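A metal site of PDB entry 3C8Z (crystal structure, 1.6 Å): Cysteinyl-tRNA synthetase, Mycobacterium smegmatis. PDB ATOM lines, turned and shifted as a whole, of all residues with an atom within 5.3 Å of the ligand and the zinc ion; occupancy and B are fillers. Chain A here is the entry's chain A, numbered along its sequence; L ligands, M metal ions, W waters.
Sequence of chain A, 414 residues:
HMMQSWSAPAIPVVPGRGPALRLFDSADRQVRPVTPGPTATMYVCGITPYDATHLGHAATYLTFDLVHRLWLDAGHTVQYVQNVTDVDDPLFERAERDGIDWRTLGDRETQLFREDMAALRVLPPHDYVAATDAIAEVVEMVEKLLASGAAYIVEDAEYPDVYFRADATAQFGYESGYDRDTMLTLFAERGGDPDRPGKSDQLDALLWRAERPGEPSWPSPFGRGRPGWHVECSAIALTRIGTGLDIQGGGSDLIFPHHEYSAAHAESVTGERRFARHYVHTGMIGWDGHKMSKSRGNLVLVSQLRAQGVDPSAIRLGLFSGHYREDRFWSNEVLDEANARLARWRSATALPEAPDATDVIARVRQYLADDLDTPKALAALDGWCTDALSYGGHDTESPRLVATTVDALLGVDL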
ATOM      1  N   TYR A  43      14.184  20.955   9.060  1.00  0.00           N
ATOM      2  CA  TYR A  43      14.594  19.950  10.014  1.00  0.00           C
ATOM      3  C   TYR A  43      13.299  19.373  10.570  1.00  0.00           C
ATOM      4  O   TYR A  43      12.451  20.145  10.999  1.00  0.00           O
ATOM      5  CB  TYR A  43      15.387  20.590  11.156  1.00  0.00           C
ATOM      6  CG  TYR A  43      15.897  19.588  12.166  1.00  0.00           C
ATOM      7  CD1 TYR A  43      17.174  19.072  12.046  1.00  0.00           C
ATOM      8  CD2 TYR A  43      15.109  19.167  13.253  1.00  0.00           C
ATOM      9  CE1 TYR A  43      17.656  18.146  12.942  1.00  0.00           C
ATOM     10  CE2 TYR A  43      15.607  18.253  14.176  1.00  0.00           C
ATOM     11  CZ  TYR A  43      16.886  17.743  14.011  1.00  0.00           C
ATOM     12  OH  TYR A  43      17.388  16.865  14.908  1.00  0.00           O
ATOM     13  N   VAL A  44      13.161  18.050  10.517  1.00  0.00           N
ATOM     14  CA  VAL A  44      11.992  17.374  11.050  1.00  0.00           C
ATOM     15  C   VAL A  44      12.454  16.359  12.082  1.00  0.00           C
ATOM     16  O   VAL A  44      13.316  15.528  11.797  1.00  0.00           O
ATOM     17  CB  VAL A  44      11.124  16.712   9.976  1.00  0.00           C
ATOM     18  CG1 VAL A  44       9.957  15.933  10.620  1.00  0.00           C
ATOM     19  CG2 VAL A  44      10.613  17.765   8.960  1.00  0.00           C
ATOM     20  N   CYS A  45      11.881  16.416  13.265  1.00  0.00           N
ATOM     21  CA  CYS A  45      12.293  15.519  14.327  1.00  0.00           C
ATOM     22  C   CYS A  45      11.983  14.067  13.979  1.00  0.00           C
ATOM     23  O   CYS A  45      10.847  13.707  13.680  1.00  0.00           O
ATOM     24  CB  CYS A  45      11.637  15.927  15.652  1.00  0.00           C
ATOM     25  SG  CYS A  45      12.393  17.358  16.379  1.00  0.00           S
ATOM     26  N   GLY A  46      13.042  13.266  14.025  1.00  0.00           N
ATOM     27  CA  GLY A  46      13.029  11.860  13.617  1.00  0.00           C
ATOM     28  C   GLY A  46      12.550  10.895  14.686  1.00  0.00           C
ATOM     29  O   GLY A  46      12.048  11.306  15.736  1.00  0.00           O
ATOM     30  N   ILE A  47      12.721   9.604  14.430  1.00  0.00           N
ATOM     31  CA  ILE A  47      12.184   8.604  15.338  1.00  0.00           C
ATOM     32  C   ILE A  47      13.130   8.306  16.496  1.00  0.00           C
ATOM     33  O   ILE A  47      14.339   8.537  16.413  1.00  0.00           O
ATOM     34  CB  ILE A  47      11.820   7.271  14.627  1.00  0.00           C
ATOM     35  CG1 ILE A  47      13.068   6.600  14.028  1.00  0.00           C
ATOM     36  CG2 ILE A  47      10.714   7.516  13.607  1.00  0.00           C
ATOM     37  CD1 ILE A  47      12.842   5.128  13.677  1.00  0.00           C
ATOM     38  N   THR A  48      12.539   7.820  17.586  1.00  0.00           N
ATOM     39  CA  THR A  48      13.283   7.108  18.631  1.00  0.00           C
ATOM     40  C   THR A  48      13.084   5.630  18.337  1.00  0.00           C
ATOM     41  O   THR A  48      11.968   5.099  18.481  1.00  0.00           O
ATOM     42  CB  THR A  48      12.761   7.474  20.023  1.00  0.00           C
ATOM     43  OG1 THR A  48      12.935   8.865  20.250  1.00  0.00           O
ATOM     44  CG2 THR A  48      13.555   6.724  21.089  1.00  0.00           C
ATOM     45  N   HIS A  54       4.626   3.296  13.453  1.00  0.00           N
ATOM     46  CA  HIS A  54       3.185   3.336  13.360  1.00  0.00           C
ATOM     47  C   HIS A  54       2.629   4.409  12.477  1.00  0.00           C
ATOM     48  O   HIS A  54       3.362   5.201  11.973  1.00  0.00           O
ATOM     49  CB  HIS A  54       2.489   3.275  14.718  1.00  0.00           C
ATOM     50  CG  HIS A  54       2.748   4.439  15.605  1.00  0.00           C
ATOM     51  ND1 HIS A  54       2.454   5.722  15.235  1.00  0.00           N
ATOM     52  CD2 HIS A  54       3.223   4.506  16.861  1.00  0.00           C
ATOM     53  CE1 HIS A  54       2.753   6.525  16.222  1.00  0.00           C
ATOM     54  NE2 HIS A  54       3.196   5.817  17.229  1.00  0.00           N
ATOM     55  N   GLY A  56       0.917   6.958  12.941  1.00  0.00           N
ATOM     56  CA  GLY A  56       1.245   8.242  13.467  1.00  0.00           C
ATOM     57  C   GLY A  56       2.556   8.805  12.972  1.00  0.00           C
ATOM     58  O   GLY A  56       2.565   9.891  12.476  1.00  0.00           O
ATOM     59  N   HIS A  57       3.643   8.068  13.185  1.00  0.00           N
ATOM     60  CA  HIS A  57       4.885   8.536  12.637  1.00  0.00           C
ATOM     61  C   HIS A  57       4.755   8.749  11.140  1.00  0.00           C
ATOM     62  O   HIS A  57       5.217   9.761  10.624  1.00  0.00           O
ATOM     63  CB  HIS A  57       5.948   7.473  12.857  1.00  0.00           C
ATOM     64  CG  HIS A  57       6.020   6.963  14.264  1.00  0.00           C
ATOM     65  ND1 HIS A  57       6.195   7.788  15.352  1.00  0.00           N
ATOM     66  CD2 HIS A  57       5.981   5.703  14.748  1.00  0.00           C
ATOM     67  CE1 HIS A  57       6.247   7.064  16.448  1.00  0.00           C
ATOM     68  NE2 HIS A  57       6.122   5.793  16.118  1.00  0.00           N
ATOM     69  N   ALA A  59       2.135   9.428   9.240  1.00  0.00           N
ATOM     70  CA  ALA A  59       1.393  10.646   8.902  1.00  0.00           C
ATOM     71  C   ALA A  59       2.243  11.896   9.034  1.00  0.00           C
ATOM     72  O   ALA A  59       2.188  12.799   8.204  1.00  0.00           O
ATOM     73  CB  ALA A  59       0.152  10.761   9.738  1.00  0.00           C
ATOM     74  N   THR A  60       3.051  11.960  10.089  1.00  0.00           N
ATOM     75  CA  THR A  60       3.924  13.100  10.285  1.00  0.00           C
ATOM     76  C   THR A  60       4.962  13.229   9.167  1.00  0.00           C
ATOM     77  O   THR A  60       5.082  14.305   8.585  1.00  0.00           O
ATOM     78  CB  THR A  60       4.538  13.051  11.677  1.00  0.00           C
ATOM     79  OG1 THR A  60       3.486  13.330  12.611  1.00  0.00           O
ATOM     80  CG2 THR A  60       5.664  14.092  11.829  1.00  0.00           C
ATOM     81  N   TYR A  61       5.650  12.146   8.810  1.00  0.00           N
ATOM     82  CA  TYR A  61       6.666  12.264   7.750  1.00  0.00           C
ATOM     83  C   TYR A  61       6.051  12.468   6.369  1.00  0.00           C
ATOM     84  O   TYR A  61       6.648  13.131   5.535  1.00  0.00           O
ATOM     85  CB  TYR A  61       7.672  11.099   7.792  1.00  0.00           C
ATOM     86  CG  TYR A  61       8.345  11.098   9.126  1.00  0.00           C
ATOM     87  CD1 TYR A  61       9.160  12.168   9.505  1.00  0.00           C
ATOM     88  CD2 TYR A  61       8.107  10.078  10.047  1.00  0.00           C
ATOM     89  CE1 TYR A  61       9.761  12.209  10.773  1.00  0.00           C
ATOM     90  CE2 TYR A  61       8.681  10.111  11.323  1.00  0.00           C
ATOM     91  CZ  TYR A  61       9.507  11.178  11.668  1.00  0.00           C
ATOM     92  OH  TYR A  61      10.057  11.202  12.928  1.00  0.00           O
ATOM     93  N   ASN A  83      16.964  13.649  12.260  1.00  0.00           N
ATOM     94  CA  ASN A  83      17.801  12.898  13.204  1.00  0.00           C
ATOM     95  C   ASN A  83      17.239  11.497  13.477  1.00  0.00           C
ATOM     96  O   ASN A  83      16.148  11.148  13.028  1.00  0.00           O
ATOM     97  CB  ASN A  83      17.824  13.658  14.539  1.00  0.00           C
ATOM     98  CG  ASN A  83      16.427  13.772  15.157  1.00  0.00           C
ATOM     99  OD1 ASN A  83      15.511  14.297  14.513  1.00  0.00           O
ATOM    100  ND2 ASN A  83      16.249  13.248  16.361  1.00  0.00           N
ATOM    101  N   THR A  85      16.959   9.578  17.275  1.00  0.00           N
ATOM    102  CA  THR A  85      17.263   9.658  18.707  1.00  0.00           C
ATOM    103  C   THR A  85      17.632   8.242  19.188  1.00  0.00           C
ATOM    104  O   THR A  85      16.822   7.539  19.818  1.00  0.00           O
ATOM    105  CB  THR A  85      16.082  10.284  19.495  1.00  0.00           C
ATOM    106  OG1 THR A  85      15.686  11.505  18.838  1.00  0.00           O
ATOM    107  CG2 THR A  85      16.509  10.589  20.922  1.00  0.00           C
ATOM    108  N   TRP A 229      17.896  15.707  25.587  1.00  0.00           N
ATOM    109  CA  TRP A 229      17.158  15.495  24.353  1.00  0.00           C
ATOM    110  C   TRP A 229      17.118  16.731  23.453  1.00  0.00           C
ATOM    111  O   TRP A 229      17.385  16.653  22.253  1.00  0.00           O
ATOM    112  CB  TRP A 229      15.744  15.027  24.727  1.00  0.00           C
ATOM    113  CG  TRP A 229      14.830  14.795  23.583  1.00  0.00           C
ATOM    114  CD1 TRP A 229      15.164  14.445  22.298  1.00  0.00           C
ATOM    115  CD2 TRP A 229      13.401  14.896  23.610  1.00  0.00           C
ATOM    116  NE1 TRP A 229      14.022  14.337  21.528  1.00  0.00           N
ATOM    117  CE2 TRP A 229      12.930  14.611  22.315  1.00  0.00           C
ATOM    118  CE3 TRP A 229      12.466  15.207  24.614  1.00  0.00           C
ATOM    119  CZ2 TRP A 229      11.567  14.615  21.992  1.00  0.00           C
ATOM    120  CZ3 TRP A 229      11.109  15.227  24.291  1.00  0.00           C
ATOM    121  CH2 TRP A 229      10.680  14.932  22.995  1.00  0.00           C
ATOM    122  N   CYS A 233      18.792  17.779  19.040  1.00  0.00           N
ATOM    123  CA  CYS A 233      18.170  18.328  17.841  1.00  0.00           C
ATOM    124  C   CYS A 233      18.633  19.750  17.515  1.00  0.00           C
ATOM    125  O   CYS A 233      18.823  20.107  16.347  1.00  0.00           O
ATOM    126  CB  CYS A 233      16.626  18.181  17.912  1.00  0.00           C
ATOM    127  SG  CYS A 233      16.136  16.482  17.820  1.00  0.00           S
ATOM    128  N   GLY A 249      10.023  21.090  12.083  1.00  0.00           N
ATOM    129  CA  GLY A 249       8.798  20.297  12.061  1.00  0.00           C
ATOM    130  C   GLY A 249       8.762  19.097  13.003  1.00  0.00           C
ATOM    131  O   GLY A 249       9.806  18.595  13.438  1.00  0.00           O
ATOM    132  N   GLY A 250       7.550  18.638  13.291  1.00  0.00           N
ATOM    133  CA  GLY A 250       7.319  17.367  13.978  1.00  0.00           C
ATOM    134  C   GLY A 250       5.887  17.295  14.447  1.00  0.00           C
ATOM    135  O   GLY A 250       5.072  18.122  14.016  1.00  0.00           O
ATOM    136  N   GLY A 251       5.588  16.326  15.300  1.00  0.00           N
ATOM    137  CA  GLY A 251       4.230  16.191  15.861  1.00  0.00           C
ATOM    138  C   GLY A 251       3.957  17.257  16.889  1.00  0.00           C
ATOM    139  O   GLY A 251       4.883  17.855  17.454  1.00  0.00           O
ATOM    140  N   SER A 252       2.671  17.544  17.110  1.00  0.00           N
ATOM    141  CA  SER A 252       2.235  18.554  18.057  1.00  0.00           C
ATOM    142  C   SER A 252       2.677  18.293  19.504  1.00  0.00           C
ATOM    143  O   SER A 252       2.795  19.267  20.272  1.00  0.00           O
ATOM    144  CB  SER A 252       0.725  18.733  17.974  1.00  0.00           C
ATOM    145  OG  SER A 252       0.403  19.467  16.807  1.00  0.00           O
ATOM    146  N   ASP A 253       2.972  17.035  19.841  1.00  0.00           N
ATOM    147  CA  ASP A 253       3.501  16.711  21.171  1.00  0.00           C
ATOM    148  C   ASP A 253       4.887  17.360  21.407  1.00  0.00           C
ATOM    149  O   ASP A 253       5.326  17.500  22.544  1.00  0.00           O
ATOM    150  CB  ASP A 253       3.565  15.187  21.415  1.00  0.00           C
ATOM    151  CG  ASP A 253       4.537  14.493  20.469  1.00  0.00           C
ATOM    152  OD1 ASP A 253       4.420  14.681  19.252  1.00  0.00           O
ATOM    153  OD2 ASP A 253       5.438  13.790  21.005  1.00  0.00           O
ATOM    154  N   LEU A 254       5.560  17.745  20.325  1.00  0.00           N
ATOM    155  CA  LEU A 254       6.883  18.379  20.436  1.00  0.00           C
ATOM    156  C   LEU A 254       6.850  19.890  20.627  1.00  0.00           C
ATOM    157  O   LEU A 254       7.891  20.533  20.840  1.00  0.00           O
ATOM    158  CB  LEU A 254       7.751  18.001  19.209  1.00  0.00           C
ATOM    159  CG  LEU A 254       7.919  16.492  19.001  1.00  0.00           C
ATOM    160  CD1 LEU A 254       8.788  16.283  17.756  1.00  0.00           C
ATOM    161  CD2 LEU A 254       8.555  15.826  20.205  1.00  0.00           C
ATOM    162  N   HIS A 258       9.913  20.142  23.796  1.00  0.00           N
ATOM    163  CA  HIS A 258      11.041  19.887  22.923  1.00  0.00           C
ATOM    164  C   HIS A 258      11.460  21.083  21.991  1.00  0.00           C
ATOM    165  O   HIS A 258      12.550  21.508  21.982  1.00  0.00           O
ATOM    166  CB  HIS A 258      10.758  18.655  22.109  1.00  0.00           C
ATOM    167  CG  HIS A 258      11.914  18.170  21.301  1.00  0.00           C
ATOM    168  ND1 HIS A 258      13.157  17.934  21.840  1.00  0.00           N
ATOM    169  CD2 HIS A 258      11.998  17.845  20.001  1.00  0.00           C
ATOM    170  CE1 HIS A 258      13.951  17.504  20.888  1.00  0.00           C
ATOM    171  NE2 HIS A 258      13.272  17.451  19.782  1.00  0.00           N
ATOM    172  N   HIS A 259      10.526  21.558  21.193  1.00  0.00           N
ATOM    173  CA  HIS A 259      10.827  22.604  20.239  1.00  0.00           C
ATOM    174  C   HIS A 259      11.086  23.974  20.880  1.00  0.00           C
ATOM    175  O   HIS A 259      11.839  24.777  20.378  1.00  0.00           O
ATOM    176  CB  HIS A 259       9.709  22.699  19.206  1.00  0.00           C
ATOM    177  CG  HIS A 259       9.720  21.566  18.252  1.00  0.00           C
ATOM    178  ND1 HIS A 259       8.732  21.339  17.332  1.00  0.00           N
ATOM    179  CD2 HIS A 259      10.626  20.584  18.078  1.00  0.00           C
ATOM    180  CE1 HIS A 259       9.029  20.265  16.651  1.00  0.00           C
ATOM    181  NE2 HIS A 259      10.173  19.792  17.071  1.00  0.00           N
ATOM    182  N   THR A 282       2.218  18.665  13.155  1.00  0.00           N
ATOM    183  CA  THR A 282       1.157  17.789  12.682  1.00  0.00           C
ATOM    184  C   THR A 282       0.235  17.358  13.807  1.00  0.00           C
ATOM    185  O   THR A 282       0.625  17.300  14.996  1.00  0.00           O
ATOM    186  CB  THR A 282       1.747  16.536  12.035  1.00  0.00           C
ATOM    187  OG1 THR A 282       2.704  15.987  12.933  1.00  0.00           O
ATOM    188  CG2 THR A 282       2.407  16.890  10.723  1.00  0.00           C
ATOM    189  N   GLY A 283      -0.987  17.016  13.421  1.00  0.00           N
ATOM    190  CA  GLY A 283      -1.953  16.428  14.337  1.00  0.00           C
ATOM    191  C   GLY A 283      -1.571  15.034  14.749  1.00  0.00           C
ATOM    192  O   GLY A 283      -0.773  14.333  14.091  1.00  0.00           O
ATOM    193  N   MET A 284      -2.158  14.583  15.851  1.00  0.00           N
ATOM    194  CA  MET A 284      -1.850  13.278  16.365  1.00  0.00           C
ATOM    195  C   MET A 284      -2.819  12.256  15.774  1.00  0.00           C
ATOM    196  O   MET A 284      -4.041  12.507  15.708  1.00  0.00           O
ATOM    197  CB  MET A 284      -1.877  13.324  17.901  1.00  0.00           C
ATOM    198  CG  MET A 284      -0.927  14.396  18.491  1.00  0.00           C
ATOM    199  SD  MET A 284       0.865  14.219  18.088  1.00  0.00           S
ATOM    200  CE  MET A 284       1.147  12.839  19.137  1.00  0.00           C
ATOM    201  N   ILE A 285      -2.273  11.134  15.294  1.00  0.00           N
ATOM    202  CA  ILE A 285      -3.085  10.017  14.784  1.00  0.00           C
ATOM    203  C   ILE A 285      -3.364   9.038  15.917  1.00  0.00           C
ATOM    204  O   ILE A 285      -2.463   8.702  16.688  1.00  0.00           O
ATOM    205  CB  ILE A 285      -2.370   9.269  13.631  1.00  0.00           C
ATOM    206  CG1 ILE A 285      -1.926  10.255  12.548  1.00  0.00           C
ATOM    207  CG2 ILE A 285      -3.286   8.178  13.018  1.00  0.00           C
ATOM    208  CD1 ILE A 285      -3.066  11.050  11.908  1.00  0.00           C
HETATM  209  N1  LIG L   1      12.909  11.167  18.591  1.00  0.00           N
HETATM  210  C1  LIG L   1      11.743  12.079  18.533  1.00  0.00           C
HETATM  211  C2  LIG L   1      11.888  13.554  18.397  1.00  0.00           C
HETATM  212  S1  LIG L   1      13.619  14.058  18.244  1.00  0.00           S
HETATM  213  C3  LIG L   1      10.392  11.544  18.827  1.00  0.00           C
HETATM  214  O1  LIG L   1       9.432  12.160  19.323  1.00  0.00           O
HETATM  215  N2  LIG L   1      10.367  10.365  18.257  1.00  0.00           N
HETATM  216  S2  LIG L   1       9.082   9.468  18.156  1.00  0.00           S
HETATM  217  O2  LIG L   1       8.391   9.357  19.459  1.00  0.00           O
HETATM  218  O3  LIG L   1       9.448   8.166  17.534  1.00  0.00           O
HETATM  219  O4  LIG L   1       8.228  10.227  17.196  1.00  0.00           O
HETATM  220  C4  LIG L   1       8.676  10.505  15.810  1.00  0.00           C
HETATM  221  C5  LIG L   1       7.708  11.562  15.562  1.00  0.00           C
HETATM  222  O5  LIG L   1       6.426  11.263  15.129  1.00  0.00           O
HETATM  223  C6  LIG L   1       7.662  13.104  15.718  1.00  0.00           C
HETATM  224  O6  LIG L   1       7.933  14.156  14.957  1.00  0.00           O
HETATM  225  C7  LIG L   1       6.641  13.089  16.728  1.00  0.00           C
HETATM  226  O7  LIG L   1       6.157  14.318  17.189  1.00  0.00           O
HETATM  227  C8  LIG L   1       5.615  12.278  15.882  1.00  0.00           C
HETATM  228  N3  LIG L   1       4.622  11.522  16.552  1.00  0.00           N
HETATM  229  C9  LIG L   1       4.668  10.745  17.649  1.00  0.00           C
HETATM  230  N4  LIG L   1       3.482  10.127  17.909  1.00  0.00           N
HETATM  231  C10 LIG L   1       2.601  10.562  16.881  1.00  0.00           C
HETATM  232  C11 LIG L   1       1.160  10.249  16.585  1.00  0.00           C
HETATM  233  N5  LIG L   1       0.458   9.453  17.403  1.00  0.00           N
HETATM  234  N6  LIG L   1       0.633  10.913  15.463  1.00  0.00           N
HETATM  235  C12 LIG L   1       1.383  11.783  14.624  1.00  0.00           C
HETATM  236  N7  LIG L   1       2.735  12.078  14.858  1.00  0.00           N
HETATM  237  C13 LIG L   1       3.331  11.429  16.019  1.00  0.00           C
HETATM  238 ZN    ZN M   1      13.797  16.475  17.960  1.00  0.00          ZN
HETATM  239  O   HOH W   1       5.616   9.558  20.926  1.00  0.00           O
HETATM  240  O   HOH W   2       6.972  11.912  20.216  1.00  0.00           O
HETATM  241  O   HOH W   3       9.180   5.573  18.261  1.00  0.00           O
HETATM  242  O   HOH W   4       0.514  13.402  11.826  1.00  0.00           O
HETATM  243  O   HOH W   5       3.368  10.765  21.041  1.00  0.00           O
HETATM  244  O   HOH W   6       5.641   7.369  19.371  1.00  0.00           O
HETATM  245  O   HOH W   7       0.991   7.939  19.685  1.00  0.00           O
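Within 4 Å of the zinc ion: Cys 45, Cys 233 and His 258. The nearest printed residue that does not touch the zinc ion is Trp 229 (4.2 Å).
The side-chain hydroxyl (OH) of Tyr 61 lies within hydrogen-bond range of the backbone carbonyl oxygen (O) of Cys 45, 2.7 Å away. SG of Cys 233 lies close to ND2 of Asn 83 (3.5 Å). SG of Cys 233 lies close to OH of Tyr 43 (3.2 Å). The side-chain hydroxyl of Thr 60 lies within hydrogen-bond range of the side-chain hydroxyl of Thr 282. The side-chain amide nitrogen (ND2) of Asn 83 is in hydrogen-bond range of the side-chain hydroxyl (OG1) of Thr 85. The side-chain hydroxyl (OH) of Tyr 61 lies close to the backbone carbonyl oxygen (O) of Gly 46 (3.4 Å). The backbone NH of Gly 56 lies within hydrogen-bond range of a ring nitrogen (ND1) of His 54. N of Ile 47 is in hydrogen-bond range of OH of Tyr 61, 3.5 Å away.
The zinc ion is bound by a ring nitrogen (NE2) of His 258 (2.1 Å), the side-chain sulfur (SG) of Cys 45 (2.3 Å), the side-chain sulfur (SG) of Cys 233 (2.3 Å) and a sulfur (S1) of the ligand (2.4 Å). The zinc ion has four donor atoms within binding distance.
Water W2 bridges OD2 of Asp 253 (2.6 Å) and O1 of the ligand (2.6 Å). Water W3 lies within hydrogen-bond range of an oxygen (O3) of the ligand (2.7 Å) and the backbone carbonyl oxygen (O) of Thr 48 (2.8 Å). Water W4 lies within hydrogen-bond range of the backbone carbonyl oxygen of Gly 283 (2.8 Å) and the side-chain hydroxyl of Thr 60 (3.1 Å).
O of Gly 56 lies close to N7 of the ligand (3.2 Å). CA of Ile 47 touches O3 of the ligand (3.5 Å). His 54 touches the ligand. OH of Tyr 61 touches C4 of the ligand, at 3.3 Å. CA of Gly 250 touches O6 of the ligand, 3.4 Å away. Leu 254 touches the ligand. Gly 283 touches the ligand. Met 284 touches the ligand. Hydrophobic or aromatic side chains within 4 Å of the ligand: Ile 47, His 54, His 57, Trp 229, Leu 254, Met 284 and Ile 285. 21 residues have an atom within 4 Å of the ligand: Cys 45, Gly 46, Ile 47, Thr 48, His 54, Gly 56, His 57, Thr 60, Tyr 61, Asn 83, Thr 85, Trp 229, Cys 233, Gly 250, Gly 251, Asp 253, Leu 254, His 258, Gly 283, Met 284 and Ile 285. The nearest printed residue that does not touch the ligand is Thr 282 (4.4 Å).
O of Cys 45 sits at hydrogen-bond distance from O6 of the ligand, at 3.2 Å. The side-chain hydroxyl (OG1) of Thr 60 is in hydrogen-bond range of a nitrogen (N7) of the ligand, at 2.7 Å. The side-chain carboxylate (OD1) of Asp 253 sits at hydrogen-bond distance from an oxygen (O7) of the ligand (2.7 Å). A nitrogen (N1) of the ligand is in hydrogen-bond range of the side-chain hydroxyl (OG1) of Thr 85, at 2.8 Å. The backbone NH of Gly 251 lies within hydrogen-bond range of an oxygen (O7) of the ligand (2.8 Å). N of Thr 48 lies within hydrogen-bond range of O3 of the ligand (3.1 Å). OG1 of Thr 48 is in hydrogen-bond range of N1 of the ligand (2.8 Å). A nitrogen (N1) of the ligand sits close to the backbone carbonyl oxygen of Gly 46, at 3.0 Å. N of Ile 285 is in hydrogen-bond range of N6 of the ligand (2.9 Å). N5 of the ligand lies within hydrogen-bond range of O of Ile 285. The indole nitrogen (NE1) of Trp 229 lies close to a sulfur (S1) of the ligand (3.3 Å). S1 of the ligand lies close to ND2 of Asn 83, 3.3 Å away. A ring nitrogen (ND1) of His 57 lies within hydrogen-bond range of an oxygen (O5) of the ligand, 3.5 Å away.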
